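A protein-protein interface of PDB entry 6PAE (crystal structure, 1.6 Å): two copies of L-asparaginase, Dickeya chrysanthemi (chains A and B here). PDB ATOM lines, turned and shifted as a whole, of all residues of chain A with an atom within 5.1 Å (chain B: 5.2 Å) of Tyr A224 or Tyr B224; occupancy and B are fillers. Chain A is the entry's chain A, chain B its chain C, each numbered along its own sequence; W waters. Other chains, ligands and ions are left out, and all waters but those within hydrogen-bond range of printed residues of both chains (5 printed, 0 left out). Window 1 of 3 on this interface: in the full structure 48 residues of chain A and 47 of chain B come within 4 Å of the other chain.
N of Ile A222 is in hydrogen-bond range of OH of Tyr B226 (3.0 Å).
The side-chain hydroxyl (OH) of Tyr A226 sits at hydrogen-bond distance from the backbone NH (N) of Ile B222 (3.0 Å).
Tyr A224 touches just these residues of chain B: Ile B222, Tyr B224 and Pro B300.
Of chain A, only Ile A222, Tyr A224 and Pro A300 come within 4 Å of Tyr B224.
Printed residues of chain A within 4 Å of Ile B222: Tyr A224 and Tyr A226.
Of the printed residues of chain A, Tyr B226 touches Ile A222.
Of the printed residues of chain A, Arg B278 touches Ala A301.
Of the printed residues of chain B, Arg A278 touches Ala B301.
Of the printed residues of chain A, Ala B301 touches Arg A278 (3.96 Å).
Asp B229 touches none of the printed residues of chain A.
Tyr A247 touches none of the printed residues of chain B.
The nearest residue of chain A that does not touch Tyr B224 is Ala A248 (4.4 Å).
Ile A222 touches Tyr B224, and with the chains exchanged Tyr A224 touches Ile B222.
Ile A222 touches Tyr B226, and with the chains exchanged Tyr A226 touches Ile B222.
Tyr A224 touches Pro B300, and with the chains exchanged Pro A300 touches Tyr B224.
Arg A278 touches Ala B301, and with the chains exchanged Ala A301 touches Arg B278.
11 positions are printed for both chains.
Of the 9 pairs that touch across the chains among the printed residues, 9 have their exchanged pair printed and touching as well.
Water W3 lies within hydrogen-bond range of O of Ile B222 (2.7 Å) and N of Tyr A224 (2.9 Å).
Water W2 lies within hydrogen-bond range of O of Ile A222 (2.7 Å) and N of Tyr B224 (2.9 Å).
Water W4 lies within hydrogen-bond range of the side-chain hydroxyl of Tyr A224 (2.7 Å) and the backbone NH of Ala B301 (3.0 Å).
Water W1 bridges OH of Tyr B224 (2.7 Å) and N of Ala A301 (2.9 Å).
Water W5 lies within hydrogen-bond range of the backbone carbonyl oxygen of Arg A278 (3.2 Å) and the backbone carbonyl oxygen of Arg B278 (3.2 Å).
Printed residues of chain B that touch a printed residue of chain A: Ile B222, Tyr B224, Tyr B226, Arg B278, Pro B300 and Ala B301.
Hydrophobic or aromatic side chains of chain B that line the printed part of chain A: Ile B222, Tyr B224, Tyr B226, Pro B300 and Ala B301.
Printed residues of chain A that touch a printed residue of chain B: Ile A222, Tyr A224, Tyr A226, Arg A278, Pro A300 and Ala A301.
Hydrophobic or aromatic side chains of chain A that line the printed part of chain B: Ile A222, Tyr A224, Tyr A226, Pro A300 and Ala A301.
NH1 of Arg A278 is in hydrogen-bond range of O of Gly A225 (2.9 Å).
The backbone carbonyl oxygen of Gly B225 lies within hydrogen-bond range of the guanidinium group of Arg B278.
Ile A222 touches Tyr B224.
CG2 of Ile B222 touches CD2 of Tyr A224, 3.6 Å away.
CD1 of Tyr A224 touches CD1 of Tyr B224, 3.5 Å away.
Pro B300 touches Tyr A224 (CB to OH, 3.8 Å).
CB of Ala B301 touches NH2 of Arg A278, at 3.96 Å.
Tyr B224 touches Pro A300.
Ala A301 touches Arg B278 (CB to NH1, 3.9 Å).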
ATOM      1  N   ILE A 222     -21.303  19.931 -27.408  1.00  0.00           N
ATOM      2  CA  ILE A 222     -21.817  21.150 -26.800  1.00  0.00           C
ATOM      3  C   ILE A 222     -21.030  21.441 -25.552  1.00  0.00           C
ATOM      4  O   ILE A 222     -20.987  20.570 -24.635  1.00  0.00           O
ATOM      5  CB  ILE A 222     -23.338  20.994 -26.505  1.00  0.00           C
ATOM      6  CG1 ILE A 222     -24.099  20.655 -27.751  1.00  0.00           C
ATOM      7  CG2 ILE A 222     -23.873  22.267 -25.861  1.00  0.00           C
ATOM      8  CD1 ILE A 222     -25.591  20.434 -27.516  1.00  0.00           C
ATOM      9  N   LEU A 223     -20.518  22.654 -25.436  1.00  0.00           N
ATOM     10  CA  LEU A 223     -19.822  23.118 -24.234  1.00  0.00           C
ATOM     11  C   LEU A 223     -20.635  24.238 -23.551  1.00  0.00           C
ATOM     12  O   LEU A 223     -21.111  25.129 -24.233  1.00  0.00           O
ATOM     13  CB  LEU A 223     -18.373  23.643 -24.484  1.00  0.00           C
ATOM     14  CG  LEU A 223     -17.522  22.488 -25.061  1.00  0.00           C
ATOM     15  CD1 LEU A 223     -16.151  23.078 -25.369  1.00  0.00           C
ATOM     16  CD2 LEU A 223     -17.424  21.385 -24.018  1.00  0.00           C
ATOM     17  N   TYR A 224     -20.713  24.199 -22.218  1.00  0.00           N
ATOM     18  CA  TYR A 224     -21.485  25.190 -21.461  1.00  0.00           C
ATOM     19  C   TYR A 224     -20.655  26.442 -21.149  1.00  0.00           C
ATOM     20  O   TYR A 224     -19.428  26.331 -21.007  1.00  0.00           O
ATOM     21  CB  TYR A 224     -22.007  24.530 -20.186  1.00  0.00           C
ATOM     22  CG  TYR A 224     -23.312  25.084 -19.637  1.00  0.00           C
ATOM     23  CD1 TYR A 224     -24.482  24.783 -20.289  1.00  0.00           C
ATOM     24  CD2 TYR A 224     -23.378  25.765 -18.437  1.00  0.00           C
ATOM     25  CE1 TYR A 224     -25.671  25.198 -19.784  1.00  0.00           C
ATOM     26  CE2 TYR A 224     -24.575  26.201 -17.933  1.00  0.00           C
ATOM     27  CZ  TYR A 224     -25.699  25.891 -18.582  1.00  0.00           C
ATOM     28  OH  TYR A 224     -26.964  26.290 -18.096  1.00  0.00           O
ATOM     29  N   GLY A 225     -21.322  27.597 -21.045  1.00  0.00           N
ATOM     30  CA  GLY A 225     -20.721  28.828 -20.574  1.00  0.00           C
ATOM     31  C   GLY A 225     -21.238  29.193 -19.156  1.00  0.00           C
ATOM     32  O   GLY A 225     -22.439  29.118 -18.847  1.00  0.00           O
ATOM     33  N   TYR A 226     -20.304  29.637 -18.302  1.00  0.00           N
ATOM     34  CA  TYR A 226     -20.476  29.862 -16.888  1.00  0.00           C
ATOM     35  C   TYR A 226     -19.194  30.483 -16.318  1.00  0.00           C
ATOM     36  O   TYR A 226     -18.134  30.414 -16.962  1.00  0.00           O
ATOM     37  CB  TYR A 226     -20.811  28.614 -16.135  1.00  0.00           C
ATOM     38  CG  TYR A 226     -19.847  27.479 -16.299  1.00  0.00           C
ATOM     39  CD1 TYR A 226     -19.873  26.721 -17.436  1.00  0.00           C
ATOM     40  CD2 TYR A 226     -19.010  27.100 -15.270  1.00  0.00           C
ATOM     41  CE1 TYR A 226     -19.067  25.623 -17.554  1.00  0.00           C
ATOM     42  CE2 TYR A 226     -18.137  26.026 -15.383  1.00  0.00           C
ATOM     43  CZ  TYR A 226     -18.188  25.275 -16.525  1.00  0.00           C
ATOM     44  OH  TYR A 226     -17.426  24.149 -16.783  1.00  0.00           O
ATOM     45  N   ASP A 229     -15.461  28.954 -16.582  1.00  0.00           N
ATOM     46  CA  ASP A 229     -15.507  27.881 -17.569  1.00  0.00           C
ATOM     47  C   ASP A 229     -14.092  27.531 -18.065  1.00  0.00           C
ATOM     48  O   ASP A 229     -13.308  28.421 -18.405  1.00  0.00           O
ATOM     49  CB  ASP A 229     -16.477  28.186 -18.740  1.00  0.00           C
ATOM     50  CG  ASP A 229     -16.092  29.405 -19.594  1.00  0.00           C
ATOM     51  OD1 ASP A 229     -15.537  30.360 -19.103  1.00  0.00           O
ATOM     52  OD2 ASP A 229     -16.350  29.380 -20.836  1.00  0.00           O
ATOM     53  N   TYR A 247     -21.686  26.218 -28.480  1.00  0.00           N
ATOM     54  CA  TYR A 247     -21.362  26.820 -27.198  1.00  0.00           C
ATOM     55  C   TYR A 247     -22.715  27.295 -26.578  1.00  0.00           C
ATOM     56  O   TYR A 247     -23.384  28.147 -27.180  1.00  0.00           O
ATOM     57  CB  TYR A 247     -20.403  27.970 -27.452  1.00  0.00           C
ATOM     58  CG  TYR A 247     -20.209  28.889 -26.286  1.00  0.00           C
ATOM     59  CD1 TYR A 247     -19.692  28.416 -25.085  1.00  0.00           C
ATOM     60  CD2 TYR A 247     -20.538  30.217 -26.357  1.00  0.00           C
ATOM     61  CE1 TYR A 247     -19.506  29.266 -23.983  1.00  0.00           C
ATOM     62  CE2 TYR A 247     -20.276  31.080 -25.306  1.00  0.00           C
ATOM     63  CZ  TYR A 247     -19.802  30.602 -24.100  1.00  0.00           C
ATOM     64  OH  TYR A 247     -19.607  31.370 -22.977  1.00  0.00           O
ATOM     65  N   ALA A 248     -23.109  26.720 -25.450  1.00  0.00           N
ATOM     66  CA  ALA A 248     -24.321  27.166 -24.725  1.00  0.00           C
ATOM     67  C   ALA A 248     -23.953  28.348 -23.875  1.00  0.00           C
ATOM     68  O   ALA A 248     -23.683  28.228 -22.674  1.00  0.00           O
ATOM     69  CB  ALA A 248     -24.879  26.034 -23.891  1.00  0.00           C
ATOM     70  N   ARG A 278     -27.269  29.590 -23.148  1.00  0.00           N
ATOM     71  CA  ARG A 278     -27.760  28.724 -22.082  1.00  0.00           C
ATOM     72  C   ARG A 278     -29.158  29.220 -21.539  1.00  0.00           C
ATOM     73  O   ARG A 278     -29.781  28.560 -20.665  1.00  0.00           O
ATOM     74  CB  ARG A 278     -26.755  28.688 -20.927  1.00  0.00           C
ATOM     75  CG  ARG A 278     -26.756  29.928 -20.001  1.00  0.00           C
ATOM     76  CD  ARG A 278     -25.666  29.861 -18.981  1.00  0.00           C
ATOM     77  NE  ARG A 278     -25.922  30.896 -17.968  1.00  0.00           N
ATOM     78  CZ  ARG A 278     -25.097  31.221 -16.983  1.00  0.00           C
ATOM     79  NH1 ARG A 278     -23.998  30.611 -16.855  1.00  0.00           N
ATOM     80  NH2 ARG A 278     -25.447  32.135 -16.063  1.00  0.00           N
ATOM     81  N   PRO A 300     -29.186  25.393 -27.814  1.00  0.00           N
ATOM     82  CA  PRO A 300     -28.018  24.572 -28.074  1.00  0.00           C
ATOM     83  C   PRO A 300     -28.327  23.217 -28.697  1.00  0.00           C
ATOM     84  O   PRO A 300     -27.599  22.758 -29.638  1.00  0.00           O
ATOM     85  CB  PRO A 300     -27.357  24.480 -26.681  1.00  0.00           C
ATOM     86  CG  PRO A 300     -27.693  25.787 -26.063  1.00  0.00           C
ATOM     87  CD  PRO A 300     -29.118  26.041 -26.497  1.00  0.00           C
ATOM     88  N   ALA A 301     -29.363  22.529 -28.217  1.00  0.00           N
ATOM     89  CA  ALA A 301     -29.702  21.177 -28.724  1.00  0.00           C
ATOM     90  C   ALA A 301     -30.116  21.329 -30.199  1.00  0.00           C
ATOM     91  O   ALA A 301     -29.742  20.471 -31.078  1.00  0.00           O
ATOM     92  CB  ALA A 301     -30.867  20.613 -27.945  1.00  0.00           C
ATOM     93  N   ILE B 222     -19.402  22.272 -15.416  1.00  0.00           N
ATOM     94  CA  ILE B 222     -20.751  21.947 -15.843  1.00  0.00           C
ATOM     95  C   ILE B 222     -20.631  21.302 -17.217  1.00  0.00           C
ATOM     96  O   ILE B 222     -20.026  21.874 -18.111  1.00  0.00           O
ATOM     97  CB  ILE B 222     -21.682  23.222 -15.956  1.00  0.00           C
ATOM     98  CG1 ILE B 222     -21.751  23.999 -14.644  1.00  0.00           C
ATOM     99  CG2 ILE B 222     -23.055  22.816 -16.438  1.00  0.00           C
ATOM    100  CD1 ILE B 222     -22.492  25.307 -14.647  1.00  0.00           C
ATOM    101  N   LEU B 223     -21.224  20.155 -17.357  1.00  0.00           N
ATOM    102  CA  LEU B 223     -21.247  19.386 -18.571  1.00  0.00           C
ATOM    103  C   LEU B 223     -22.694  19.287 -19.039  1.00  0.00           C
ATOM    104  O   LEU B 223     -23.581  18.979 -18.267  1.00  0.00           O
ATOM    105  CB  LEU B 223     -20.638  17.956 -18.416  1.00  0.00           C
ATOM    106  CG  LEU B 223     -19.192  17.980 -17.912  1.00  0.00           C
ATOM    107  CD1 LEU B 223     -18.703  16.554 -17.796  1.00  0.00           C
ATOM    108  CD2 LEU B 223     -18.276  18.725 -18.885  1.00  0.00           C
ATOM    109  N   TYR B 224     -22.856  19.436 -20.328  1.00  0.00           N
ATOM    110  CA  TYR B 224     -24.193  19.401 -20.969  1.00  0.00           C
ATOM    111  C   TYR B 224     -24.636  18.003 -21.320  1.00  0.00           C
ATOM    112  O   TYR B 224     -23.800  17.149 -21.700  1.00  0.00           O
ATOM    113  CB  TYR B 224     -24.173  20.246 -22.223  1.00  0.00           C
ATOM    114  CG  TYR B 224     -25.468  20.921 -22.586  1.00  0.00           C
ATOM    115  CD1 TYR B 224     -25.938  21.941 -21.795  1.00  0.00           C
ATOM    116  CD2 TYR B 224     -26.196  20.589 -23.726  1.00  0.00           C
ATOM    117  CE1 TYR B 224     -27.064  22.613 -22.094  1.00  0.00           C
ATOM    118  CE2 TYR B 224     -27.373  21.317 -24.060  1.00  0.00           C
ATOM    119  CZ  TYR B 224     -27.784  22.323 -23.243  1.00  0.00           C
ATOM    120  OH  TYR B 224     -28.968  23.050 -23.561  1.00  0.00           O
ATOM    121  N   GLY B 225     -25.949  17.802 -21.380  1.00  0.00           N
ATOM    122  CA  GLY B 225     -26.557  16.490 -21.732  1.00  0.00           C
ATOM    123  C   GLY B 225     -27.316  16.684 -23.041  1.00  0.00           C
ATOM    124  O   GLY B 225     -28.061  17.669 -23.181  1.00  0.00           O
ATOM    125  N   TYR B 226     -27.139  15.748 -23.971  1.00  0.00           N
ATOM    126  CA  TYR B 226     -27.699  15.857 -25.303  1.00  0.00           C
ATOM    127  C   TYR B 226     -27.409  14.534 -26.024  1.00  0.00           C
ATOM    128  O   TYR B 226     -26.576  13.733 -25.535  1.00  0.00           O
ATOM    129  CB  TYR B 226     -27.072  16.981 -26.084  1.00  0.00           C
ATOM    130  CG  TYR B 226     -25.538  16.967 -26.162  1.00  0.00           C
ATOM    131  CD1 TYR B 226     -24.756  17.400 -25.120  1.00  0.00           C
ATOM    132  CD2 TYR B 226     -24.895  16.628 -27.347  1.00  0.00           C
ATOM    133  CE1 TYR B 226     -23.356  17.414 -25.209  1.00  0.00           C
ATOM    134  CE2 TYR B 226     -23.492  16.602 -27.442  1.00  0.00           C
ATOM    135  CZ  TYR B 226     -22.746  17.022 -26.400  1.00  0.00           C
ATOM    136  OH  TYR B 226     -21.383  17.086 -26.418  1.00  0.00           O
ATOM    137  N   ASP B 229     -23.901  12.586 -26.367  1.00  0.00           N
ATOM    138  CA  ASP B 229     -22.986  13.288 -25.481  1.00  0.00           C
ATOM    139  C   ASP B 229     -21.782  12.371 -25.094  1.00  0.00           C
ATOM    140  O   ASP B 229     -21.971  11.214 -24.903  1.00  0.00           O
ATOM    141  CB  ASP B 229     -23.690  13.799 -24.243  1.00  0.00           C
ATOM    142  CG  ASP B 229     -24.367  12.689 -23.393  1.00  0.00           C
ATOM    143  OD1 ASP B 229     -24.711  11.577 -23.786  1.00  0.00           O
ATOM    144  OD2 ASP B 229     -24.716  13.050 -22.260  1.00  0.00           O
ATOM    145  N   TYR B 247     -24.209  18.409 -13.909  1.00  0.00           N
ATOM    146  CA  TYR B 247     -24.681  17.902 -15.191  1.00  0.00           C
ATOM    147  C   TYR B 247     -25.959  18.667 -15.587  1.00  0.00           C
ATOM    148  O   TYR B 247     -26.967  18.571 -14.873  1.00  0.00           O
ATOM    149  CB  TYR B 247     -24.951  16.442 -15.024  1.00  0.00           C
ATOM    150  CG  TYR B 247     -25.630  15.746 -16.168  1.00  0.00           C
ATOM    151  CD1 TYR B 247     -25.100  15.752 -17.463  1.00  0.00           C
ATOM    152  CD2 TYR B 247     -26.822  15.083 -15.971  1.00  0.00           C
ATOM    153  CE1 TYR B 247     -25.754  15.083 -18.510  1.00  0.00           C
ATOM    154  CE2 TYR B 247     -27.482  14.434 -16.980  1.00  0.00           C
ATOM    155  CZ  TYR B 247     -26.935  14.406 -18.247  1.00  0.00           C
ATOM    156  OH  TYR B 247     -27.604  13.833 -19.302  1.00  0.00           O
ATOM    157  N   ALA B 248     -25.878  19.380 -16.704  1.00  0.00           N
ATOM    158  CA  ALA B 248     -27.073  20.078 -17.297  1.00  0.00           C
ATOM    159  C   ALA B 248     -27.782  19.084 -18.153  1.00  0.00           C
ATOM    160  O   ALA B 248     -27.680  19.039 -19.377  1.00  0.00           O
ATOM    161  CB  ALA B 248     -26.665  21.333 -18.044  1.00  0.00           C
ATOM    162  N   ARG B 278     -30.968  20.876 -18.292  1.00  0.00           N
ATOM    163  CA  ARG B 278     -30.778  21.895 -19.322  1.00  0.00           C
ATOM    164  C   ARG B 278     -32.114  22.601 -19.654  1.00  0.00           C
ATOM    165  O   ARG B 278     -32.110  23.513 -20.490  1.00  0.00           O
ATOM    166  CB  ARG B 278     -30.261  21.255 -20.618  1.00  0.00           C
ATOM    167  CG  ARG B 278     -31.290  20.449 -21.405  1.00  0.00           C
ATOM    168  CD  ARG B 278     -30.679  19.739 -22.607  1.00  0.00           C
ATOM    169  NE  ARG B 278     -31.745  19.231 -23.492  1.00  0.00           N
ATOM    170  CZ  ARG B 278     -31.587  18.516 -24.578  1.00  0.00           C
ATOM    171  NH1 ARG B 278     -30.394  18.130 -24.961  1.00  0.00           N
ATOM    172  NH2 ARG B 278     -32.683  18.212 -25.318  1.00  0.00           N
ATOM    173  N   PRO B 300     -28.418  24.769 -13.685  1.00  0.00           N
ATOM    174  CA  PRO B 300     -27.009  24.321 -13.583  1.00  0.00           C
ATOM    175  C   PRO B 300     -26.094  25.407 -13.019  1.00  0.00           C
ATOM    176  O   PRO B 300     -25.210  25.095 -12.187  1.00  0.00           O
ATOM    177  CB  PRO B 300     -26.689  23.968 -15.059  1.00  0.00           C
ATOM    178  CG  PRO B 300     -27.994  23.533 -15.605  1.00  0.00           C
ATOM    179  CD  PRO B 300     -29.020  24.375 -14.942  1.00  0.00           C
ATOM    180  N   ALA B 301     -26.329  26.679 -13.394  1.00  0.00           N
ATOM    181  CA  ALA B 301     -25.425  27.751 -12.944  1.00  0.00           C
ATOM    182  C   ALA B 301     -25.550  27.937 -11.437  1.00  0.00           C
ATOM    183  O   ALA B 301     -24.549  28.097 -10.710  1.00  0.00           O
ATOM    184  CB  ALA B 301     -25.803  29.045 -13.618  1.00  0.00           C
HETATM  185  O   HOH W   1     -30.695  23.092 -25.678  1.00  0.00           O
HETATM  186  O   HOH W   2     -20.547  19.924 -22.056  1.00  0.00           O
HETATM  187  O   HOH W   3     -19.433  22.051 -20.732  1.00  0.00           O
HETATM  188  O   HOH W   4     -27.802  27.538 -15.831  1.00  0.00           O
HETATM  189  O   HOH W   5     -32.393  26.720 -20.508  1.00  0.00           O
